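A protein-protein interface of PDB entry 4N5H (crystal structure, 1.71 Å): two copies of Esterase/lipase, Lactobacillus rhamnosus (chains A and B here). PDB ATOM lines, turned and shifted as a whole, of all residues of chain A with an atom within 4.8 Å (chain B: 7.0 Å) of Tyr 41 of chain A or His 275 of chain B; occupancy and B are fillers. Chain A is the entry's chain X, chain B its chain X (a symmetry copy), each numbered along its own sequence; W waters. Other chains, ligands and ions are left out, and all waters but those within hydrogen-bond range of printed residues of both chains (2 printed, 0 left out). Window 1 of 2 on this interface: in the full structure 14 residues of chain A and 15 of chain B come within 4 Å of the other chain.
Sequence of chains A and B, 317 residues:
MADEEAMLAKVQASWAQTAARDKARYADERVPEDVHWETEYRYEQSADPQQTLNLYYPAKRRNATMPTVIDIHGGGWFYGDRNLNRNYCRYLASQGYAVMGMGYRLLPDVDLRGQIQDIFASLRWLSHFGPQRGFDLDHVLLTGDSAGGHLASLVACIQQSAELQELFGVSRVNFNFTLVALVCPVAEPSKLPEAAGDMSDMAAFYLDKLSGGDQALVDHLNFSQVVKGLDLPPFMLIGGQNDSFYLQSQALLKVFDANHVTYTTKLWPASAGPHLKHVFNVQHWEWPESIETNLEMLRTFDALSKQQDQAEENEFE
Water W2 lies within hydrogen-bond range of the backbone carbonyl oxygen (O) of Pro 274 of chain B (2.7 Å) and the guanidinium group (NH1) of Arg 42 of chain A (3.0 Å). Water W1 lies within hydrogen-bond range of the backbone carbonyl oxygen (O) of His 275 of chain B and the backbone NH (N) of Arg 42 of chain A.
OE1 of Glu 38 of chain A is in hydrogen-bond range of OH of Tyr 41 of chain A, at 2.7 Å. O of Leu 53 of chain A lies within hydrogen-bond range of N of Glu 40 of chain A (3.2 Å). The backbone carbonyl oxygen of Tyr 41 of chain A is in hydrogen-bond range of the backbone NH of Leu 53 of chain A (2.9 Å). NE of Arg 133 of chain A is in hydrogen-bond range of O of Phe 129 of chain A. The side-chain carboxylate of Glu 286 of chain B lies within hydrogen-bond range of a ring nitrogen (ND1) of His 284 of chain B, at 2.9 Å. A ring nitrogen (ND1) of His 284 of chain B sits close to the indole nitrogen (NE1) of Trp 287 of chain B (3.5 Å).
Of the 15 printed residues of chain B, 11 touch a printed residue of chain A. Hydrophobic or aromatic side chains of chain A that line the printed part of chain B: Tyr 41, Trp 125 and Phe 129. Among the printed residues, 23 pairs touch across the chains. Among the printed residues, Asp or Glu carboxylates within 4 Å of a Lys or Arg side-chain nitrogen of the other chain: Arg 133 of chain A with Glu 289 of chain B (2.8 Å).
ND1 of His 284 of chain B sits close to O of Thr 39 of chain A. The backbone NH of Thr 39 of chain A sits at hydrogen-bond distance from the side-chain carboxylate of Glu 286 of chain B, at 3.2 Å. The backbone carbonyl oxygen (O) of Thr 39 of chain A sits at hydrogen-bond distance from the indole nitrogen (NE1) of Trp 287 of chain B. A ring nitrogen (NE2) of His 284 of chain B is in hydrogen-bond range of the side-chain carboxylate (OE1) of Glu 40 of chain A (2.7 Å). The indole nitrogen (NE1) of Trp 125 of chain A lies within hydrogen-bond range of a ring nitrogen (ND1) of His 275 of chain B. OE2 of Glu 289 of chain B lies within salt-bridge range of NH2 of Arg 133 of chain A (2.8 Å).
No position is printed for both chains. Of the 23 pairs that touch across the chains among the printed residues, none has its exchanged pair printed and touching as well.
Among the printed residues, merely in contact across the chains: Glu 38 of chain A with Glu 286 of chain B, Glu 38 of chain A with Trp 287 of chain B, Glu 38 of chain A with Pro 288 of chain B, Glu 40 of chain A with Trp 287 of chain B, Tyr 41 of chain A with His 275 of chain B, Tyr 41 of chain A with Trp 287 of chain B, Tyr 41 of chain A with Pro 288 of chain B, Arg 42 of chain A with Pro 274 of chain B, Arg 42 of chain A with His 275 of chain B, Arg 42 of chain A with Lys 277 of chain B, Tyr 43 of chain A with Pro 274 of chain B, Trp 125 of chain A with Pro 274 of chain B, Phe 129 of chain A with Ser 271 of chain B, Phe 129 of chain A with Ala 272 of chain B, Phe 129 of chain A with Gly 273 of chain B, Phe 129 of chain A with His 275 of chain B and Arg 133 of chain A with Pro 288 of chain B.
Of the printed residues of chain B, Glu 38 of chain A touches Glu 286, Trp 287 and Pro 288. Gln 51 of chain A touches none of the printed residues of chain B. His 275 of chain B touches four residues of chain A. Leu 276 of chain B touches none of the printed residues of chain A. Of the printed residues of chain A, Glu 286 of chain B touches Glu 38 and Thr 39.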
ATOM      1  N   GLU A  38     -14.813  -5.716  19.453  1.00  0.00           N
ATOM      2  CA  GLU A  38     -14.996  -5.689  18.041  1.00  0.00           C
ATOM      3  C   GLU A  38     -13.575  -5.496  17.479  1.00  0.00           C
ATOM      4  O   GLU A  38     -12.922  -4.533  17.804  1.00  0.00           O
ATOM      5  CB  GLU A  38     -15.867  -4.477  17.674  1.00  0.00           C
ATOM      6  CG  GLU A  38     -17.301  -4.546  18.192  1.00  0.00           C
ATOM      7  CD  GLU A  38     -18.042  -3.213  18.185  1.00  0.00           C
ATOM      8  OE1 GLU A  38     -17.466  -2.180  17.778  1.00  0.00           O
ATOM      9  OE2 GLU A  38     -19.194  -3.132  18.749  1.00  0.00           O
ATOM     10  N   THR A  39     -13.171  -6.406  16.626  1.00  0.00           N
ATOM     11  CA  THR A  39     -11.760  -6.476  16.284  1.00  0.00           C
ATOM     12  C   THR A  39     -11.456  -6.132  14.832  1.00  0.00           C
ATOM     13  O   THR A  39     -12.323  -6.306  13.942  1.00  0.00           O
ATOM     14  CB  THR A  39     -11.177  -7.871  16.608  1.00  0.00           C
ATOM     15  OG1 THR A  39     -11.918  -8.883  15.945  1.00  0.00           O
ATOM     16  CG2 THR A  39     -11.193  -8.115  18.086  1.00  0.00           C
ATOM     17  N   GLU A  40     -10.183  -5.773  14.608  1.00  0.00           N
ATOM     18  CA  GLU A  40      -9.640  -5.737  13.249  1.00  0.00           C
ATOM     19  C   GLU A  40     -10.341  -4.760  12.301  1.00  0.00           C
ATOM     20  O   GLU A  40     -10.578  -4.988  11.119  1.00  0.00           O
ATOM     21  CB  GLU A  40      -9.647  -7.205  12.676  1.00  0.00           C
ATOM     22  CG  GLU A  40      -8.656  -7.349  11.494  1.00  0.00           C
ATOM     23  CD  GLU A  40      -8.851  -8.693  10.787  1.00  0.00           C
ATOM     24  OE1 GLU A  40      -9.967  -9.315  10.814  1.00  0.00           O
ATOM     25  OE2 GLU A  40      -7.909  -9.106  10.035  1.00  0.00           O
ATOM     26  N   TYR A  41     -10.686  -3.581  12.807  1.00  0.00           N
ATOM     27  CA  TYR A  41     -11.152  -2.585  11.929  1.00  0.00           C
ATOM     28  C   TYR A  41      -9.982  -1.899  11.212  1.00  0.00           C
ATOM     29  O   TYR A  41      -9.052  -1.372  11.863  1.00  0.00           O
ATOM     30  CB  TYR A  41     -11.823  -1.495  12.732  1.00  0.00           C
ATOM     31  CG  TYR A  41     -13.157  -1.711  13.365  1.00  0.00           C
ATOM     32  CD1 TYR A  41     -13.289  -2.041  14.740  1.00  0.00           C
ATOM     33  CD2 TYR A  41     -14.309  -1.552  12.639  1.00  0.00           C
ATOM     34  CE1 TYR A  41     -14.518  -2.147  15.337  1.00  0.00           C
ATOM     35  CE2 TYR A  41     -15.545  -1.673  13.247  1.00  0.00           C
ATOM     36  CZ  TYR A  41     -15.618  -1.913  14.597  1.00  0.00           C
ATOM     37  OH  TYR A  41     -16.904  -1.941  15.170  1.00  0.00           O
ATOM     38  N   ARG A  42     -10.058  -1.817   9.873  1.00  0.00           N
ATOM     39  CA  ARG A  42      -9.065  -1.002   9.203  1.00  0.00           C
ATOM     40  C   ARG A  42      -9.382   0.454   9.481  1.00  0.00           C
ATOM     41  O   ARG A  42     -10.506   0.904   9.302  1.00  0.00           O
ATOM     42  CB  ARG A  42      -9.178  -1.230   7.683  1.00  0.00           C
ATOM     43  CG  ARG A  42      -8.648  -2.538   7.178  1.00  0.00           C
ATOM     44  CD  ARG A  42      -8.940  -2.665   5.692  1.00  0.00           C
ATOM     45  NE  ARG A  42      -8.420  -3.915   5.227  1.00  0.00           N
ATOM     46  CZ  ARG A  42      -8.356  -4.248   3.933  1.00  0.00           C
ATOM     47  NH1 ARG A  42      -8.677  -3.362   3.010  1.00  0.00           N
ATOM     48  NH2 ARG A  42      -7.803  -5.429   3.605  1.00  0.00           N
ATOM     49  N   TYR A  43      -8.371   1.247   9.793  1.00  0.00           N
ATOM     50  CA  TYR A  43      -8.618   2.665   9.970  1.00  0.00           C
ATOM     51  C   TYR A  43      -8.190   3.582   8.770  1.00  0.00           C
ATOM     52  O   TYR A  43      -8.377   4.793   8.844  1.00  0.00           O
ATOM     53  CB  TYR A  43      -8.040   3.211  11.318  1.00  0.00           C
ATOM     54  CG  TYR A  43      -6.604   2.979  11.615  1.00  0.00           C
ATOM     55  CD1 TYR A  43      -5.643   3.662  10.892  1.00  0.00           C
ATOM     56  CD2 TYR A  43      -6.157   2.052  12.591  1.00  0.00           C
ATOM     57  CE1 TYR A  43      -4.330   3.550  11.204  1.00  0.00           C
ATOM     58  CE2 TYR A  43      -4.819   1.914  12.863  1.00  0.00           C
ATOM     59  CZ  TYR A  43      -3.914   2.639  12.183  1.00  0.00           C
ATOM     60  OH  TYR A  43      -2.526   2.448  12.449  1.00  0.00           O
ATOM     61  N   GLN A  51      -2.325  -1.423  10.476  1.00  0.00           N
ATOM     62  CA  GLN A  51      -3.194  -0.207  10.399  1.00  0.00           C
ATOM     63  C   GLN A  51      -4.677  -0.592  10.690  1.00  0.00           C
ATOM     64  O   GLN A  51      -5.611  -0.310   9.902  1.00  0.00           O
ATOM     65  CB  GLN A  51      -2.988   0.532   9.092  1.00  0.00           C
ATOM     66  CG  GLN A  51      -1.530   1.071   8.980  1.00  0.00           C
ATOM     67  CD  GLN A  51      -1.226   1.719   7.638  1.00  0.00           C
ATOM     68  OE1 GLN A  51      -1.596   1.158   6.598  1.00  0.00           O
ATOM     69  NE2 GLN A  51      -0.702   2.948   7.644  1.00  0.00           N
ATOM     70  N   THR A  52      -4.796  -1.254  11.795  1.00  0.00           N
ATOM     71  CA  THR A  52      -6.068  -1.754  12.289  1.00  0.00           C
ATOM     72  C   THR A  52      -6.213  -1.433  13.777  1.00  0.00           C
ATOM     73  O   THR A  52      -5.251  -1.117  14.459  1.00  0.00           O
ATOM     74  CB  THR A  52      -6.219  -3.306  12.092  1.00  0.00           C
ATOM     75  OG1 THR A  52      -5.127  -3.952  12.743  1.00  0.00           O
ATOM     76  CG2 THR A  52      -6.287  -3.643  10.615  1.00  0.00           C
ATOM     77  N   LEU A  53      -7.425  -1.531  14.259  1.00  0.00           N
ATOM     78  CA  LEU A  53      -7.733  -1.212  15.704  1.00  0.00           C
ATOM     79  C   LEU A  53      -8.777  -2.175  16.244  1.00  0.00           C
ATOM     80  O   LEU A  53      -9.536  -2.796  15.472  1.00  0.00           O
ATOM     81  CB  LEU A  53      -8.061   0.281  15.941  1.00  0.00           C
ATOM     82  CG  LEU A  53      -9.231   0.815  15.141  1.00  0.00           C
ATOM     83  CD1 LEU A  53     -10.582   0.481  15.807  1.00  0.00           C
ATOM     84  CD2 LEU A  53      -9.217   2.316  15.067  1.00  0.00           C
ATOM     85  N   LEU A  55     -11.897  -2.290  19.347  1.00  0.00           N
ATOM     86  CA  LEU A  55     -12.810  -1.574  20.265  1.00  0.00           C
ATOM     87  C   LEU A  55     -13.303  -2.527  21.338  1.00  0.00           C
ATOM     88  O   LEU A  55     -13.692  -3.680  21.095  1.00  0.00           O
ATOM     89  CB  LEU A  55     -14.005  -0.977  19.543  1.00  0.00           C
ATOM     90  CG  LEU A  55     -13.664  -0.120  18.290  1.00  0.00           C
ATOM     91  CD1 LEU A  55     -14.895   0.386  17.613  1.00  0.00           C
ATOM     92  CD2 LEU A  55     -12.752   1.042  18.665  1.00  0.00           C
ATOM     93  N   TRP A 125     -10.364   8.157  12.477  1.00  0.00           N
ATOM     94  CA  TRP A 125     -11.368   7.138  12.323  1.00  0.00           C
ATOM     95  C   TRP A 125     -12.368   7.160  13.467  1.00  0.00           C
ATOM     96  O   TRP A 125     -13.590   7.156  13.271  1.00  0.00           O
ATOM     97  CB  TRP A 125     -10.691   5.771  12.231  1.00  0.00           C
ATOM     98  CG  TRP A 125     -11.647   4.667  11.852  1.00  0.00           C
ATOM     99  CD1 TRP A 125     -11.912   4.185  10.603  1.00  0.00           C
ATOM    100  CD2 TRP A 125     -12.444   3.907  12.740  1.00  0.00           C
ATOM    101  NE1 TRP A 125     -12.825   3.186  10.654  1.00  0.00           N
ATOM    102  CE2 TRP A 125     -13.131   2.937  11.964  1.00  0.00           C
ATOM    103  CE3 TRP A 125     -12.597   3.892  14.135  1.00  0.00           C
ATOM    104  CZ2 TRP A 125     -14.039   2.048  12.525  1.00  0.00           C
ATOM    105  CZ3 TRP A 125     -13.468   2.967  14.669  1.00  0.00           C
ATOM    106  CH2 TRP A 125     -14.202   2.106  13.876  1.00  0.00           C
ATOM    107  N   PHE A 129     -16.483   7.474  13.378  1.00  0.00           N
ATOM    108  CA  PHE A 129     -17.250   6.261  13.578  1.00  0.00           C
ATOM    109  C   PHE A 129     -17.531   5.890  15.011  1.00  0.00           C
ATOM    110  O   PHE A 129     -18.335   5.003  15.314  1.00  0.00           O
ATOM    111  CB  PHE A 129     -16.569   5.107  12.761  1.00  0.00           C
ATOM    112  CG  PHE A 129     -16.414   5.443  11.330  1.00  0.00           C
ATOM    113  CD1 PHE A 129     -15.173   5.639  10.817  1.00  0.00           C
ATOM    114  CD2 PHE A 129     -17.508   5.700  10.526  1.00  0.00           C
ATOM    115  CE1 PHE A 129     -14.949   6.061   9.518  1.00  0.00           C
ATOM    116  CE2 PHE A 129     -17.309   6.097   9.220  1.00  0.00           C
ATOM    117  CZ  PHE A 129     -16.021   6.274   8.702  1.00  0.00           C
ATOM    118  N   ARG A 133     -21.263   4.133  17.706  1.00  0.00           N
ATOM    119  CA  ARG A 133     -21.190   2.825  18.346  1.00  0.00           C
ATOM    120  C   ARG A 133     -20.832   2.873  19.809  1.00  0.00           C
ATOM    121  O   ARG A 133     -20.484   1.856  20.435  1.00  0.00           O
ATOM    122  CB  ARG A 133     -20.243   1.917  17.529  1.00  0.00           C
ATOM    123  CG  ARG A 133     -18.808   2.253  17.632  1.00  0.00           C
ATOM    124  CD  ARG A 133     -17.972   1.624  16.449  1.00  0.00           C
ATOM    125  NE  ARG A 133     -18.343   2.244  15.183  1.00  0.00           N
ATOM    126  CZ  ARG A 133     -18.629   1.646  14.060  1.00  0.00           C
ATOM    127  NH1 ARG A 133     -18.440   0.315  13.902  1.00  0.00           N
ATOM    128  NH2 ARG A 133     -19.061   2.379  13.086  1.00  0.00           N
ATOM    129  N   ASN B 242     -16.094   0.579  -0.702  1.00  0.00           N
ATOM    130  CA  ASN B 242     -14.814   0.145  -0.243  1.00  0.00           C
ATOM    131  C   ASN B 242     -14.557  -1.363  -0.402  1.00  0.00           C
ATOM    132  O   ASN B 242     -13.546  -1.880   0.048  1.00  0.00           O
ATOM    133  CB  ASN B 242     -14.546   0.618   1.212  1.00  0.00           C
ATOM    134  CG  ASN B 242     -13.897   1.990   1.225  1.00  0.00           C
ATOM    135  OD1 ASN B 242     -12.843   2.158   0.631  1.00  0.00           O
ATOM    136  ND2 ASN B 242     -14.551   2.967   1.804  1.00  0.00           N
ATOM    137  N   SER B 271     -18.058   6.983   2.308  1.00  0.00           N
ATOM    138  CA  SER B 271     -18.115   7.826   3.498  1.00  0.00           C
ATOM    139  C   SER B 271     -18.379   7.051   4.768  1.00  0.00           C
ATOM    140  O   SER B 271     -18.055   7.538   5.877  1.00  0.00           O
ATOM    141  CB  SER B 271     -19.192   8.928   3.284  1.00  0.00           C
ATOM    142  OG  SER B 271     -20.469   8.382   3.135  1.00  0.00           O
ATOM    143  N   ALA B 272     -18.968   5.849   4.663  1.00  0.00           N
ATOM    144  CA  ALA B 272     -19.192   4.997   5.836  1.00  0.00           C
ATOM    145  C   ALA B 272     -17.923   4.272   6.324  1.00  0.00           C
ATOM    146  O   ALA B 272     -17.898   3.626   7.399  1.00  0.00           O
ATOM    147  CB  ALA B 272     -20.253   3.937   5.564  1.00  0.00           C
ATOM    148  N   GLY B 273     -16.822   4.447   5.650  1.00  0.00           N
ATOM    149  CA  GLY B 273     -15.550   4.167   6.233  1.00  0.00           C
ATOM    150  C   GLY B 273     -14.690   3.099   5.501  1.00  0.00           C
ATOM    151  O   GLY B 273     -15.201   2.213   4.836  1.00  0.00           O
ATOM    152  N   PRO B 274     -13.385   3.123   5.740  1.00  0.00           N
ATOM    153  CA  PRO B 274     -12.492   2.242   5.096  1.00  0.00           C
ATOM    154  C   PRO B 274     -12.528   0.798   5.627  1.00  0.00           C
ATOM    155  O   PRO B 274     -11.959  -0.135   5.014  1.00  0.00           O
ATOM    156  CB  PRO B 274     -11.154   2.883   5.411  1.00  0.00           C
ATOM    157  CG  PRO B 274     -11.317   3.501   6.722  1.00  0.00           C
ATOM    158  CD  PRO B 274     -12.681   4.071   6.637  1.00  0.00           C
ATOM    159  N   HIS B 275     -13.094   0.644   6.839  1.00  0.00           N
ATOM    160  CA  HIS B 275     -13.200  -0.671   7.417  1.00  0.00           C
ATOM    161  C   HIS B 275     -14.240  -1.555   6.729  1.00  0.00           C
ATOM    162  O   HIS B 275     -14.211  -2.791   6.908  1.00  0.00           O
ATOM    163  CB  HIS B 275     -13.509  -0.545   8.922  1.00  0.00           C
ATOM    164  CG  HIS B 275     -14.717   0.266   9.218  1.00  0.00           C
ATOM    165  ND1 HIS B 275     -14.786   1.632   8.965  1.00  0.00           N
ATOM    166  CD2 HIS B 275     -15.922  -0.072   9.727  1.00  0.00           C
ATOM    167  CE1 HIS B 275     -15.951   2.091   9.362  1.00  0.00           C
ATOM    168  NE2 HIS B 275     -16.654   1.080   9.835  1.00  0.00           N
ATOM    169  N   LEU B 276     -15.142  -0.956   5.929  1.00  0.00           N
ATOM    170  CA  LEU B 276     -16.243  -1.722   5.282  1.00  0.00           C
ATOM    171  C   LEU B 276     -15.685  -2.284   3.987  1.00  0.00           C
ATOM    172  O   LEU B 276     -16.101  -1.969   2.858  1.00  0.00           O
ATOM    173  CB  LEU B 276     -17.405  -0.778   5.065  1.00  0.00           C
ATOM    174  CG  LEU B 276     -17.944  -0.221   6.345  1.00  0.00           C
ATOM    175  CD1 LEU B 276     -19.178   0.563   6.002  1.00  0.00           C
ATOM    176  CD2 LEU B 276     -18.233  -1.265   7.411  1.00  0.00           C
ATOM    177  N   LYS B 277     -14.728  -3.172   4.202  1.00  0.00           N
ATOM    178  CA  LYS B 277     -13.981  -3.819   3.129  1.00  0.00           C
ATOM    179  C   LYS B 277     -14.757  -4.992   2.520  1.00  0.00           C
ATOM    180  O   LYS B 277     -15.866  -5.272   2.890  1.00  0.00           O
ATOM    181  CB  LYS B 277     -12.667  -4.333   3.694  1.00  0.00           C
ATOM    182  CG  LYS B 277     -12.802  -5.446   4.759  1.00  0.00           C
ATOM    183  CD  LYS B 277     -11.473  -6.102   5.100  1.00  0.00           C
ATOM    184  CE  LYS B 277     -11.055  -7.092   3.998  1.00  0.00           C
ATOM    185  NZ  LYS B 277     -11.825  -8.349   3.815  1.00  0.00           N
ATOM    186  N   HIS B 278     -14.120  -5.679   1.553  1.00  0.00           N
ATOM    187  CA  HIS B 278     -14.698  -6.891   0.959  1.00  0.00           C
ATOM    188  C   HIS B 278     -15.161  -7.803   2.041  1.00  0.00           C
ATOM    189  O   HIS B 278     -14.434  -8.128   2.961  1.00  0.00           O
ATOM    190  CB  HIS B 278     -13.563  -7.566   0.144  1.00  0.00           C
ATOM    191  CG  HIS B 278     -13.998  -8.740  -0.652  1.00  0.00           C
ATOM    192  ND1 HIS B 278     -14.902  -8.624  -1.686  1.00  0.00           N
ATOM    193  CD2 HIS B 278     -13.593 -10.029  -0.636  1.00  0.00           C
ATOM    194  CE1 HIS B 278     -15.104  -9.826  -2.206  1.00  0.00           C
ATOM    195  NE2 HIS B 278     -14.283 -10.676  -1.635  1.00  0.00           N
ATOM    196  N   PHE B 280     -17.026  -7.653   4.617  1.00  0.00           N
ATOM    197  CA  PHE B 280     -16.783  -7.295   6.037  1.00  0.00           C
ATOM    198  C   PHE B 280     -17.840  -7.884   6.948  1.00  0.00           C
ATOM    199  O   PHE B 280     -17.524  -8.294   8.057  1.00  0.00           O
ATOM    200  CB  PHE B 280     -16.698  -5.753   6.242  1.00  0.00           C
ATOM    201  CG  PHE B 280     -18.054  -5.102   6.186  1.00  0.00           C
ATOM    202  CD1 PHE B 280     -18.874  -5.037   7.309  1.00  0.00           C
ATOM    203  CD2 PHE B 280     -18.557  -4.561   4.964  1.00  0.00           C
ATOM    204  CE1 PHE B 280     -20.167  -4.489   7.203  1.00  0.00           C
ATOM    205  CE2 PHE B 280     -19.788  -3.981   4.862  1.00  0.00           C
ATOM    206  CZ  PHE B 280     -20.641  -3.945   6.011  1.00  0.00           C
ATOM    207  N   HIS B 284     -16.655 -10.163  10.115  1.00  0.00           N
ATOM    208  CA  HIS B 284     -16.858  -9.591  11.455  1.00  0.00           C
ATOM    209  C   HIS B 284     -18.313  -9.363  11.741  1.00  0.00           C
ATOM    210  O   HIS B 284     -18.854  -8.200  11.667  1.00  0.00           O
ATOM    211  CB  HIS B 284     -16.103  -8.281  11.559  1.00  0.00           C
ATOM    212  CG  HIS B 284     -14.645  -8.477  11.783  1.00  0.00           C
ATOM    213  ND1 HIS B 284     -14.145  -8.800  13.024  1.00  0.00           N
ATOM    214  CD2 HIS B 284     -13.628  -8.562  10.936  1.00  0.00           C
ATOM    215  CE1 HIS B 284     -12.831  -9.020  12.916  1.00  0.00           C
ATOM    216  NE2 HIS B 284     -12.512  -8.890  11.650  1.00  0.00           N
ATOM    217  N   GLU B 286     -19.712  -9.126  14.400  1.00  0.00           N
ATOM    218  CA  GLU B 286     -19.977  -8.405  15.637  1.00  0.00           C
ATOM    219  C   GLU B 286     -19.964  -6.881  15.423  1.00  0.00           C
ATOM    220  O   GLU B 286     -20.361  -6.129  16.291  1.00  0.00           O
ATOM    221  CB  GLU B 286     -18.925  -8.864  16.694  1.00  0.00           C
ATOM    222  CG  GLU B 286     -17.517  -8.251  16.617  1.00  0.00           C
ATOM    223  CD  GLU B 286     -16.589  -8.828  15.566  1.00  0.00           C
ATOM    224  OE1 GLU B 286     -17.033  -9.647  14.704  1.00  0.00           O
ATOM    225  OE2 GLU B 286     -15.426  -8.457  15.552  1.00  0.00           O
ATOM    226  N   TRP B 287     -19.454  -6.409  14.287  1.00  0.00           N
ATOM    227  CA  TRP B 287     -19.415  -4.983  14.134  1.00  0.00           C
ATOM    228  C   TRP B 287     -20.873  -4.466  13.958  1.00  0.00           C
ATOM    229  O   TRP B 287     -21.676  -5.062  13.237  1.00  0.00           O
ATOM    230  CB  TRP B 287     -18.680  -4.586  12.922  1.00  0.00           C
ATOM    231  CG  TRP B 287     -17.237  -4.939  12.873  1.00  0.00           C
ATOM    232  CD1 TRP B 287     -16.472  -5.424  13.847  1.00  0.00           C
ATOM    233  CD2 TRP B 287     -16.382  -4.664  11.755  1.00  0.00           C
ATOM    234  NE1 TRP B 287     -15.171  -5.513  13.411  1.00  0.00           N
ATOM    235  CE2 TRP B 287     -15.088  -5.070  12.122  1.00  0.00           C
ATOM    236  CE3 TRP B 287     -16.609  -4.118  10.465  1.00  0.00           C
ATOM    237  CZ2 TRP B 287     -13.999  -5.039  11.229  1.00  0.00           C
ATOM    238  CZ3 TRP B 287     -15.510  -4.030   9.574  1.00  0.00           C
ATOM    239  CH2 TRP B 287     -14.224  -4.467   9.969  1.00  0.00           C
ATOM    240  N   PRO B 288     -21.172  -3.234  14.449  1.00  0.00           N
ATOM    241  CA  PRO B 288     -22.515  -2.624  14.223  1.00  0.00           C
ATOM    242  C   PRO B 288     -22.982  -2.582  12.770  1.00  0.00           C
ATOM    243  O   PRO B 288     -24.126  -2.924  12.475  1.00  0.00           O
ATOM    244  CB  PRO B 288     -22.316  -1.189  14.764  1.00  0.00           C
ATOM    245  CG  PRO B 288     -21.229  -1.315  15.783  1.00  0.00           C
ATOM    246  CD  PRO B 288     -20.355  -2.462  15.413  1.00  0.00           C
ATOM    247  N   GLU B 289     -22.113  -2.277  11.824  1.00  0.00           N
ATOM    248  CA  GLU B 289     -22.535  -2.276  10.411  1.00  0.00           C
ATOM    249  C   GLU B 289     -22.838  -3.647   9.853  1.00  0.00           C
ATOM    250  O   GLU B 289     -23.662  -3.836   8.967  1.00  0.00           O
ATOM    251  CB  GLU B 289     -21.490  -1.618   9.532  1.00  0.00           C
ATOM    252  CG  GLU B 289     -21.149  -0.128   9.791  1.00  0.00           C
ATOM    253  CD  GLU B 289     -20.006   0.053  10.755  1.00  0.00           C
ATOM    254  OE1 GLU B 289     -19.707  -0.831  11.609  1.00  0.00           O
ATOM    255  OE2 GLU B 289     -19.382   1.123  10.614  1.00  0.00           O
HETATM  256  O   HOH W   1     -11.646  -3.420   7.909  1.00  0.00           O
HETATM  257  O   HOH W   2     -10.106  -0.763   3.111  1.00  0.00           O
